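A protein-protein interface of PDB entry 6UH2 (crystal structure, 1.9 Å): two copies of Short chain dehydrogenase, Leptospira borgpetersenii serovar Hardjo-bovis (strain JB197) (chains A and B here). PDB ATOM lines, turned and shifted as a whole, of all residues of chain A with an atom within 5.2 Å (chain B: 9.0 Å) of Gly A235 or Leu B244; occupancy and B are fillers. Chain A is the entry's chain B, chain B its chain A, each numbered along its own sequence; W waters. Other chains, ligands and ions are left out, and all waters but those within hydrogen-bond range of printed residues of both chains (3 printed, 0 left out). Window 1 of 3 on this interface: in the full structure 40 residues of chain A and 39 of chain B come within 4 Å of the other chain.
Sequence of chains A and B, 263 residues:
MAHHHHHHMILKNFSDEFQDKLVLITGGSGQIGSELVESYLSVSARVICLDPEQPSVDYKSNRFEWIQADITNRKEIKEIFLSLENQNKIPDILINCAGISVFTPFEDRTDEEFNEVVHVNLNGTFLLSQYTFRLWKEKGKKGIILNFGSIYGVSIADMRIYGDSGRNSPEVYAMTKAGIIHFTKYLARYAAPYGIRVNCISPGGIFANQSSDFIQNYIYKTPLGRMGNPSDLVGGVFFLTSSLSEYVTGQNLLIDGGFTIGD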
ATOM      1  N   PHE A  14      -1.513  -7.150  11.669  1.00  0.00           N
ATOM      2  CA  PHE A  14      -0.929  -8.387  12.179  1.00  0.00           C
ATOM      3  C   PHE A  14      -1.779  -9.021  13.276  1.00  0.00           C
ATOM      4  O   PHE A  14      -1.896 -10.249  13.334  1.00  0.00           O
ATOM      5  CB  PHE A  14       0.491  -8.126  12.678  1.00  0.00           C
ATOM      6  CG  PHE A  14       1.460  -7.829  11.573  1.00  0.00           C
ATOM      7  CD1 PHE A  14       1.365  -8.498  10.361  1.00  0.00           C
ATOM      8  CD2 PHE A  14       2.450  -6.873  11.730  1.00  0.00           C
ATOM      9  CE1 PHE A  14       2.245  -8.222   9.326  1.00  0.00           C
ATOM     10  CE2 PHE A  14       3.332  -6.594  10.704  1.00  0.00           C
ATOM     11  CZ  PHE A  14       3.229  -7.270   9.500  1.00  0.00           C
ATOM     12  N   SER A 231      14.701  -7.881  17.945  1.00  0.00           N
ATOM     13  CA  SER A 231      13.546  -7.123  17.470  1.00  0.00           C
ATOM     14  C   SER A 231      13.700  -6.684  16.010  1.00  0.00           C
ATOM     15  O   SER A 231      12.691  -6.473  15.323  1.00  0.00           O
ATOM     16  CB  SER A 231      13.313  -5.911  18.379  1.00  0.00           C
ATOM     17  OG  SER A 231      14.489  -5.120  18.444  1.00  0.00           O
ATOM     18  N   ASP A 232      14.945  -6.534  15.519  1.00  0.00           N
ATOM     19  CA  ASP A 232      15.175  -6.208  14.108  1.00  0.00           C
ATOM     20  C   ASP A 232      14.632  -7.270  13.167  1.00  0.00           C
ATOM     21  O   ASP A 232      14.476  -6.997  11.971  1.00  0.00           O
ATOM     22  CB  ASP A 232      16.675  -6.049  13.792  1.00  0.00           C
ATOM     23  CG  ASP A 232      17.298  -4.845  14.480  1.00  0.00           C
ATOM     24  OD1 ASP A 232      16.627  -3.796  14.557  1.00  0.00           O
ATOM     25  OD2 ASP A 232      18.457  -4.957  14.941  1.00  0.00           O
ATOM     26  N   LEU A 233      14.368  -8.475  13.668  1.00  0.00           N
ATOM     27  CA  LEU A 233      13.936  -9.573  12.815  1.00  0.00           C
ATOM     28  C   LEU A 233      12.428  -9.725  12.757  1.00  0.00           C
ATOM     29  O   LEU A 233      11.928 -10.379  11.837  1.00  0.00           O
ATOM     30  CB  LEU A 233      14.549 -10.896  13.298  1.00  0.00           C
ATOM     31  CG  LEU A 233      16.073 -10.887  13.395  1.00  0.00           C
ATOM     32  CD1 LEU A 233      16.567 -12.168  14.029  1.00  0.00           C
ATOM     33  CD2 LEU A 233      16.696 -10.700  12.015  1.00  0.00           C
ATOM     34  N   VAL A 234      11.699  -9.118  13.695  1.00  0.00           N
ATOM     35  CA  VAL A 234      10.274  -9.424  13.841  1.00  0.00           C
ATOM     36  C   VAL A 234       9.501  -8.982  12.604  1.00  0.00           C
ATOM     37  O   VAL A 234       8.588  -9.680  12.142  1.00  0.00           O
ATOM     38  CB  VAL A 234       9.719  -8.773  15.123  1.00  0.00           C
ATOM     39  CG1 VAL A 234       8.196  -8.943  15.214  1.00  0.00           C
ATOM     40  CG2 VAL A 234      10.399  -9.349  16.371  1.00  0.00           C
ATOM     41  N   GLY A 235       9.848  -7.815  12.053  1.00  0.00           N
ATOM     42  CA  GLY A 235       9.121  -7.316  10.894  1.00  0.00           C
ATOM     43  C   GLY A 235       9.165  -8.281   9.723  1.00  0.00           C
ATOM     44  O   GLY A 235       8.129  -8.623   9.148  1.00  0.00           O
ATOM     45  N   GLY A 236      10.365  -8.754   9.377  1.00  0.00           N
ATOM     46  CA  GLY A 236      10.493  -9.707   8.282  1.00  0.00           C
ATOM     47  C   GLY A 236       9.863 -11.058   8.589  1.00  0.00           C
ATOM     48  O   GLY A 236       9.286 -11.700   7.702  1.00  0.00           O
ATOM     49  N   VAL A 237       9.974 -11.516   9.841  1.00  0.00           N
ATOM     50  CA  VAL A 237       9.266 -12.734  10.252  1.00  0.00           C
ATOM     51  C   VAL A 237       7.766 -12.573  10.029  1.00  0.00           C
ATOM     52  O   VAL A 237       7.114 -13.437   9.430  1.00  0.00           O
ATOM     53  CB  VAL A 237       9.588 -13.080  11.719  1.00  0.00           C
ATOM     54  CG1 VAL A 237       8.657 -14.196  12.235  1.00  0.00           C
ATOM     55  CG2 VAL A 237      11.068 -13.501  11.869  1.00  0.00           C
ATOM     56  N   PHE A 238       7.196 -11.456  10.501  1.00  0.00           N
ATOM     57  CA  PHE A 238       5.769 -11.209  10.299  1.00  0.00           C
ATOM     58  C   PHE A 238       5.440 -11.073   8.817  1.00  0.00           C
ATOM     59  O   PHE A 238       4.430 -11.610   8.342  1.00  0.00           O
ATOM     60  CB  PHE A 238       5.331  -9.944  11.052  1.00  0.00           C
ATOM     61  CG  PHE A 238       5.061 -10.156  12.532  1.00  0.00           C
ATOM     62  CD1 PHE A 238       5.345 -11.370  13.150  1.00  0.00           C
ATOM     63  CD2 PHE A 238       4.510  -9.137  13.295  1.00  0.00           C
ATOM     64  CE1 PHE A 238       5.091 -11.555  14.507  1.00  0.00           C
ATOM     65  CE2 PHE A 238       4.239  -9.317  14.659  1.00  0.00           C
ATOM     66  CZ  PHE A 238       4.539 -10.531  15.261  1.00  0.00           C
ATOM     67  N   PHE A 239       6.278 -10.354   8.069  1.00  0.00           N
ATOM     68  CA  PHE A 239       6.049 -10.211   6.634  1.00  0.00           C
ATOM     69  C   PHE A 239       5.938 -11.570   5.953  1.00  0.00           C
ATOM     70  O   PHE A 239       4.977 -11.837   5.216  1.00  0.00           O
ATOM     71  CB  PHE A 239       7.173  -9.386   6.007  1.00  0.00           C
ATOM     72  CG  PHE A 239       7.112  -9.323   4.505  1.00  0.00           C
ATOM     73  CD1 PHE A 239       6.049  -8.706   3.872  1.00  0.00           C
ATOM     74  CD2 PHE A 239       8.124  -9.888   3.728  1.00  0.00           C
ATOM     75  CE1 PHE A 239       5.985  -8.638   2.479  1.00  0.00           C
ATOM     76  CE2 PHE A 239       8.072  -9.822   2.335  1.00  0.00           C
ATOM     77  CZ  PHE A 239       7.000  -9.198   1.715  1.00  0.00           C
ATOM     78  N   LEU A 240       6.908 -12.453   6.193  1.00  0.00           N
ATOM     79  CA  LEU A 240       6.963 -13.721   5.468  1.00  0.00           C
ATOM     80  C   LEU A 240       5.984 -14.765   6.001  1.00  0.00           C
ATOM     81  O   LEU A 240       5.836 -15.829   5.390  1.00  0.00           O
ATOM     82  CB  LEU A 240       8.386 -14.299   5.505  1.00  0.00           C
ATOM     83  CG  LEU A 240       9.465 -13.489   4.759  1.00  0.00           C
ATOM     84  CD1 LEU A 240      10.878 -14.041   5.007  1.00  0.00           C
ATOM     85  CD2 LEU A 240       9.162 -13.508   3.262  1.00  0.00           C
ATOM     86  N   ASN B  13      -1.475   1.049  13.207  1.00  0.00           N
ATOM     87  CA  ASN B  13      -1.833   0.709  11.836  1.00  0.00           C
ATOM     88  C   ASN B  13      -0.717   1.167  10.904  1.00  0.00           C
ATOM     89  O   ASN B  13       0.175   1.921  11.298  1.00  0.00           O
ATOM     90  CB  ASN B  13      -3.168   1.355  11.432  1.00  0.00           C
ATOM     91  N   PHE B  14      -0.759   0.713   9.647  1.00  0.00           N
ATOM     92  CA  PHE B  14       0.184   1.267   8.681  1.00  0.00           C
ATOM     93  C   PHE B  14      -0.024   2.763   8.507  1.00  0.00           C
ATOM     94  O   PHE B  14       0.904   3.462   8.084  1.00  0.00           O
ATOM     95  CB  PHE B  14       0.087   0.558   7.324  1.00  0.00           C
ATOM     96  CG  PHE B  14       0.997  -0.634   7.194  1.00  0.00           C
ATOM     97  CD1 PHE B  14       2.372  -0.477   7.200  1.00  0.00           C
ATOM     98  CD2 PHE B  14       0.479  -1.906   7.052  1.00  0.00           C
ATOM     99  CE1 PHE B  14       3.218  -1.564   7.087  1.00  0.00           C
ATOM    100  CE2 PHE B  14       1.320  -3.002   6.932  1.00  0.00           C
ATOM    101  CZ  PHE B  14       2.694  -2.829   6.949  1.00  0.00           C
ATOM    102  N   GLU B  17       2.502   4.188  10.607  1.00  0.00           N
ATOM    103  CA  GLU B  17       3.792   4.229   9.924  1.00  0.00           C
ATOM    104  C   GLU B  17       3.864   5.407   8.962  1.00  0.00           C
ATOM    105  O   GLU B  17       4.835   6.170   8.972  1.00  0.00           O
ATOM    106  CB  GLU B  17       4.049   2.927   9.158  1.00  0.00           C
ATOM    107  CG  GLU B  17       4.452   1.740  10.007  1.00  0.00           C
ATOM    108  CD  GLU B  17       5.881   1.826  10.524  1.00  0.00           C
ATOM    109  OE1 GLU B  17       6.680   2.645  10.013  1.00  0.00           O
ATOM    110  OE2 GLU B  17       6.201   1.055  11.449  1.00  0.00           O
ATOM    111  N   PHE B  18       2.843   5.570   8.120  1.00  0.00           N
ATOM    112  CA  PHE B  18       2.973   6.390   6.925  1.00  0.00           C
ATOM    113  C   PHE B  18       2.186   7.691   6.949  1.00  0.00           C
ATOM    114  O   PHE B  18       2.382   8.514   6.047  1.00  0.00           O
ATOM    115  CB  PHE B  18       2.554   5.584   5.686  1.00  0.00           C
ATOM    116  CG  PHE B  18       3.488   4.434   5.359  1.00  0.00           C
ATOM    117  CD1 PHE B  18       4.833   4.665   5.119  1.00  0.00           C
ATOM    118  CD2 PHE B  18       3.016   3.133   5.282  1.00  0.00           C
ATOM    119  CE1 PHE B  18       5.688   3.629   4.816  1.00  0.00           C
ATOM    120  CE2 PHE B  18       3.874   2.082   4.978  1.00  0.00           C
ATOM    121  CZ  PHE B  18       5.214   2.331   4.744  1.00  0.00           C
ATOM    122  N   ILE B 144      14.396   6.716   2.674  1.00  0.00           N
ATOM    123  CA  ILE B 144      14.418   5.336   2.193  1.00  0.00           C
ATOM    124  C   ILE B 144      14.159   5.340   0.692  1.00  0.00           C
ATOM    125  O   ILE B 144      13.215   5.987   0.226  1.00  0.00           O
ATOM    126  CB  ILE B 144      13.370   4.457   2.901  1.00  0.00           C
ATOM    127  CG1 ILE B 144      13.596   4.440   4.424  1.00  0.00           C
ATOM    128  CG2 ILE B 144      13.373   3.035   2.286  1.00  0.00           C
ATOM    129  CD1 ILE B 144      12.371   3.897   5.216  1.00  0.00           C
ATOM    130  N   ARG B 197      18.495   4.155   3.724  1.00  0.00           N
ATOM    131  CA  ARG B 197      18.373   2.758   3.300  1.00  0.00           C
ATOM    132  C   ARG B 197      17.925   2.672   1.848  1.00  0.00           C
ATOM    133  O   ARG B 197      17.165   3.514   1.374  1.00  0.00           O
ATOM    134  CB  ARG B 197      17.379   1.986   4.165  1.00  0.00           C
ATOM    135  CG  ARG B 197      17.753   1.957   5.643  1.00  0.00           C
ATOM    136  CD  ARG B 197      16.996   0.842   6.342  1.00  0.00           C
ATOM    137  NE  ARG B 197      15.593   1.173   6.647  1.00  0.00           N
ATOM    138  CZ  ARG B 197      14.535   0.582   6.100  1.00  0.00           C
ATOM    139  NH1 ARG B 197      14.685  -0.366   5.166  1.00  0.00           N
ATOM    140  NH2 ARG B 197      13.313   0.933   6.494  1.00  0.00           N
ATOM    141  N   VAL B 234       2.220  -4.871  -2.785  1.00  0.00           N
ATOM    142  CA  VAL B 234       2.054  -3.777  -1.824  1.00  0.00           C
ATOM    143  C   VAL B 234       2.667  -4.128  -0.473  1.00  0.00           C
ATOM    144  O   VAL B 234       3.303  -3.277   0.168  1.00  0.00           O
ATOM    145  CB  VAL B 234       0.568  -3.407  -1.677  1.00  0.00           C
ATOM    146  CG1 VAL B 234       0.407  -2.341  -0.584  1.00  0.00           C
ATOM    147  CG2 VAL B 234       0.017  -2.892  -3.003  1.00  0.00           C
ATOM    148  N   GLY B 235       2.473  -5.369  -0.009  1.00  0.00           N
ATOM    149  CA  GLY B 235       3.023  -5.763   1.281  1.00  0.00           C
ATOM    150  C   GLY B 235       4.533  -5.619   1.341  1.00  0.00           C
ATOM    151  O   GLY B 235       5.083  -5.093   2.318  1.00  0.00           O
ATOM    152  N   GLY B 236       5.228  -6.069   0.295  1.00  0.00           N
ATOM    153  CA  GLY B 236       6.676  -5.932   0.283  1.00  0.00           C
ATOM    154  C   GLY B 236       7.110  -4.486   0.169  1.00  0.00           C
ATOM    155  O   GLY B 236       8.113  -4.076   0.763  1.00  0.00           O
ATOM    156  N   VAL B 237       6.379  -3.700  -0.617  1.00  0.00           N
ATOM    157  CA  VAL B 237       6.669  -2.271  -0.717  1.00  0.00           C
ATOM    158  C   VAL B 237       6.545  -1.610   0.657  1.00  0.00           C
ATOM    159  O   VAL B 237       7.449  -0.890   1.104  1.00  0.00           O
ATOM    160  CB  VAL B 237       5.736  -1.614  -1.752  1.00  0.00           C
ATOM    161  CG1 VAL B 237       5.777  -0.098  -1.613  1.00  0.00           C
ATOM    162  CG2 VAL B 237       6.146  -2.024  -3.159  1.00  0.00           C
ATOM    163  N   PHE B 238       5.421  -1.846   1.343  1.00  0.00           N
ATOM    164  CA  PHE B 238       5.250  -1.306   2.690  1.00  0.00           C
ATOM    165  C   PHE B 238       6.319  -1.834   3.641  1.00  0.00           C
ATOM    166  O   PHE B 238       6.865  -1.075   4.453  1.00  0.00           O
ATOM    167  CB  PHE B 238       3.846  -1.623   3.232  1.00  0.00           C
ATOM    168  CG  PHE B 238       2.770  -0.679   2.743  1.00  0.00           C
ATOM    169  CD1 PHE B 238       2.989   0.134   1.636  1.00  0.00           C
ATOM    170  CD2 PHE B 238       1.547  -0.616   3.389  1.00  0.00           C
ATOM    171  CE1 PHE B 238       2.019   1.003   1.200  1.00  0.00           C
ATOM    172  CE2 PHE B 238       0.558   0.249   2.950  1.00  0.00           C
ATOM    173  CZ  PHE B 238       0.792   1.061   1.859  1.00  0.00           C
ATOM    174  N   PHE B 239       6.635  -3.129   3.558  1.00  0.00           N
ATOM    175  CA  PHE B 239       7.667  -3.697   4.427  1.00  0.00           C
ATOM    176  C   PHE B 239       8.985  -2.951   4.270  1.00  0.00           C
ATOM    177  O   PHE B 239       9.578  -2.498   5.259  1.00  0.00           O
ATOM    178  CB  PHE B 239       7.860  -5.188   4.135  1.00  0.00           C
ATOM    179  CG  PHE B 239       9.065  -5.795   4.831  1.00  0.00           C
ATOM    180  CD1 PHE B 239       9.107  -5.897   6.211  1.00  0.00           C
ATOM    181  CD2 PHE B 239      10.154  -6.267   4.094  1.00  0.00           C
ATOM    182  CE1 PHE B 239      10.225  -6.434   6.859  1.00  0.00           C
ATOM    183  CE2 PHE B 239      11.263  -6.818   4.730  1.00  0.00           C
ATOM    184  CZ  PHE B 239      11.293  -6.910   6.119  1.00  0.00           C
ATOM    185  N   LEU B 240       9.442  -2.786   3.030  1.00  0.00           N
ATOM    186  CA  LEU B 240      10.752  -2.197   2.761  1.00  0.00           C
ATOM    187  C   LEU B 240      10.789  -0.681   2.925  1.00  0.00           C
ATOM    188  O   LEU B 240      11.882  -0.100   2.894  1.00  0.00           O
ATOM    189  CB  LEU B 240      11.210  -2.566   1.344  1.00  0.00           C
ATOM    190  CG  LEU B 240      11.590  -4.042   1.169  1.00  0.00           C
ATOM    191  CD1 LEU B 240      11.881  -4.344  -0.295  1.00  0.00           C
ATOM    192  CD2 LEU B 240      12.788  -4.435   2.042  1.00  0.00           C
ATOM    193  N   THR B 241       9.652  -0.015   3.111  1.00  0.00           N
ATOM    194  CA  THR B 241       9.670   1.432   3.308  1.00  0.00           C
ATOM    195  C   THR B 241       9.183   1.843   4.686  1.00  0.00           C
ATOM    196  O   THR B 241       8.934   3.034   4.908  1.00  0.00           O
ATOM    197  CB  THR B 241       8.840   2.144   2.234  1.00  0.00           C
ATOM    198  OG1 THR B 241       7.501   1.640   2.262  1.00  0.00           O
ATOM    199  CG2 THR B 241       9.451   1.912   0.837  1.00  0.00           C
ATOM    200  N   SER B 242       9.045   0.900   5.616  1.00  0.00           N
ATOM    201  CA  SER B 242       8.531   1.175   6.963  1.00  0.00           C
ATOM    202  C   SER B 242       9.574   0.792   8.013  1.00  0.00           C
ATOM    203  O   SER B 242      10.611   0.216   7.702  1.00  0.00           O
ATOM    204  CB  SER B 242       7.233   0.406   7.220  1.00  0.00           C
ATOM    205  OG  SER B 242       7.508  -0.986   7.329  1.00  0.00           O
ATOM    206  N   SER B 243       9.268   1.092   9.280  1.00  0.00           N
ATOM    207  CA  SER B 243      10.133   0.698  10.388  1.00  0.00           C
ATOM    208  C   SER B 243      10.234  -0.815  10.554  1.00  0.00           C
ATOM    209  O   SER B 243      11.104  -1.281  11.295  1.00  0.00           O
ATOM    210  CB  SER B 243       9.622   1.309  11.692  1.00  0.00           C
ATOM    211  OG  SER B 243       8.403   0.699  12.061  1.00  0.00           O
ATOM    212  N   LEU B 244       9.364  -1.588   9.899  1.00  0.00           N
ATOM    213  CA  LEU B 244       9.466  -3.045   9.955  1.00  0.00           C
ATOM    214  C   LEU B 244      10.784  -3.557   9.401  1.00  0.00           C
ATOM    215  O   LEU B 244      11.167  -4.699   9.697  1.00  0.00           O
ATOM    216  CB  LEU B 244       8.320  -3.695   9.176  1.00  0.00           C
ATOM    217  CG  LEU B 244       6.880  -3.465   9.656  1.00  0.00           C
ATOM    218  CD1 LEU B 244       5.916  -4.044   8.623  1.00  0.00           C
ATOM    219  CD2 LEU B 244       6.627  -4.069  11.039  1.00  0.00           C
ATOM    220  N   SER B 245      11.472  -2.761   8.582  1.00  0.00           N
ATOM    221  CA  SER B 245      12.703  -3.196   7.925  1.00  0.00           C
ATOM    222  C   SER B 245      13.887  -2.293   8.256  1.00  0.00           C
ATOM    223  O   SER B 245      14.800  -2.153   7.441  1.00  0.00           O
ATOM    224  CB  SER B 245      12.513  -3.276   6.407  1.00  0.00           C
ATOM    225  OG  SER B 245      12.170  -2.009   5.857  1.00  0.00           O
ATOM    226  N   GLU B 246      13.906  -1.715   9.466  1.00  0.00           N
ATOM    227  CA  GLU B 246      14.969  -0.789   9.871  1.00  0.00           C
ATOM    228  C   GLU B 246      16.382  -1.315   9.627  1.00  0.00           C
ATOM    229  O   GLU B 246      17.296  -0.524   9.362  1.00  0.00           O
ATOM    230  CB  GLU B 246      14.855  -0.457  11.365  1.00  0.00           C
ATOM    231  CG  GLU B 246      13.769   0.501  11.710  1.00  0.00           C
ATOM    232  CD  GLU B 246      13.795   0.913  13.185  1.00  0.00           C
ATOM    233  OE1 GLU B 246      14.354   0.168  14.027  1.00  0.00           O
ATOM    234  OE2 GLU B 246      13.248   1.991  13.490  1.00  0.00           O
ATOM    235  N   TYR B 247      16.598  -2.620   9.784  1.00  0.00           N
ATOM    236  CA  TYR B 247      17.928  -3.216   9.664  1.00  0.00           C
ATOM    237  C   TYR B 247      18.143  -3.899   8.312  1.00  0.00           C
ATOM    238  O   TYR B 247      19.073  -4.701   8.166  1.00  0.00           O
ATOM    239  CB  TYR B 247      18.149  -4.206  10.812  1.00  0.00           C
ATOM    240  CG  TYR B 247      19.592  -4.520  11.157  1.00  0.00           C
ATOM    241  CD1 TYR B 247      20.523  -3.499  11.387  1.00  0.00           C
ATOM    242  CD2 TYR B 247      20.014  -5.840  11.305  1.00  0.00           C
ATOM    243  CE1 TYR B 247      21.852  -3.797  11.720  1.00  0.00           C
ATOM    244  CE2 TYR B 247      21.327  -6.150  11.645  1.00  0.00           C
ATOM    245  CZ  TYR B 247      22.239  -5.126  11.855  1.00  0.00           C
ATOM    246  OH  TYR B 247      23.538  -5.437  12.179  1.00  0.00           O
ATOM    247  N   VAL B 248      17.308  -3.590   7.319  1.00  0.00           N
ATOM    248  CA  VAL B 248      17.387  -4.209   5.996  1.00  0.00           C
ATOM    249  C   VAL B 248      17.845  -3.141   5.012  1.00  0.00           C
ATOM    250  O   VAL B 248      17.140  -2.145   4.803  1.00  0.00           O
ATOM    251  CB  VAL B 248      16.036  -4.805   5.560  1.00  0.00           C
ATOM    252  CG1 VAL B 248      16.169  -5.497   4.199  1.00  0.00           C
ATOM    253  CG2 VAL B 248      15.492  -5.777   6.611  1.00  0.00           C
HETATM  254  O   HOH W   1      14.566  -4.578  10.514  1.00  0.00           O
HETATM  255  O   HOH W   2      14.191  -2.702  14.284  1.00  0.00           O
HETATM  256  O   HOH W   3      12.608  -7.185   9.926  1.00  0.00           O
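Printed residues of chain A that touch a printed residue of chain B: Asp A232, Gly A235, Gly A236 and Phe A239. Of the 21 printed residues of chain B, 5 touch a printed residue of chain A. Hydrophobic or aromatic side chains of chain B that line the printed part of chain A: Phe B239 and Tyr B247.
Of the printed residues of chain B, Asp A232 touches Tyr B247. No residue of chain B comes within 4 Å of Val A234. Gly A235 touches just these residues of chain B: Phe B239 and Leu B244. Of chain B, only Phe B239 comes within 4 Å of Gly A236. Of the printed residues of chain B, Phe A239 touches Gly B235, Gly B236 and Phe B239. Leu A240 touches none of the printed residues of chain B. Of the printed residues of chain A, Gly B235 touches Phe A239. Of the printed residues of chain A, Gly B236 touches Phe A239 (3.5 Å). Of the printed residues of chain A, Phe B239 touches Gly A235 (3.6 Å), Gly A236 (3.4 Å) and Phe A239 (3.97 Å). Thr B241 touches none of the printed residues of chain A. The nearest printed residue of chain A that does not touch Leu B244 is Gly A236 (4.1 Å). The nearest printed residue of chain A that does not touch Phe B239 is Val A237 (5.9 Å).
O of Phe B239 sits at hydrogen-bond distance from OG of Ser B242 (3.3 Å). The backbone carbonyl oxygen of Phe B239 is in hydrogen-bond range of the side-chain hydroxyl of Ser B245, at 2.7 Å. OG of Ser B242 sits close to N of Leu B244 (3.2 Å).
Asp A232 touches Tyr B247. Gly A235 touches Phe B239 (C to CE1, 3.6 Å). Gly A235 touches Leu B244 (CA to O, 3.5 Å). Gly A236 touches Phe B239. CE1 of Phe A239 touches C of Gly B235, 3.5 Å away. Phe A239 touches Gly B236 (CE1 to N, 3.5 Å). Phe B239 touches Phe A239.
Water W2 lies within hydrogen-bond range of OD1 of Asp A232 (2.7 Å) and OE1 of Glu B246 (2.9 Å). Water W3 lies within hydrogen-bond range of O of Asp A232 (2.8 Å), N of Gly A236 (2.8 Å) and O of Leu B244 (2.9 Å). Water W1 lies within hydrogen-bond range of O of Asp A232 (2.8 Å), N of Tyr B247 (2.9 Å), N of Glu B246 (3.1 Å) and O of Leu B244 (3.5 Å).
Gly A235 touches Phe B239, and with the chains exchanged Phe A239 touches Gly B235. Gly A236 touches Phe B239, and with the chains exchanged Phe A239 touches Gly B236. Phe B239 touches its own counterpart, Phe A239. 8 positions are printed for both chains.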
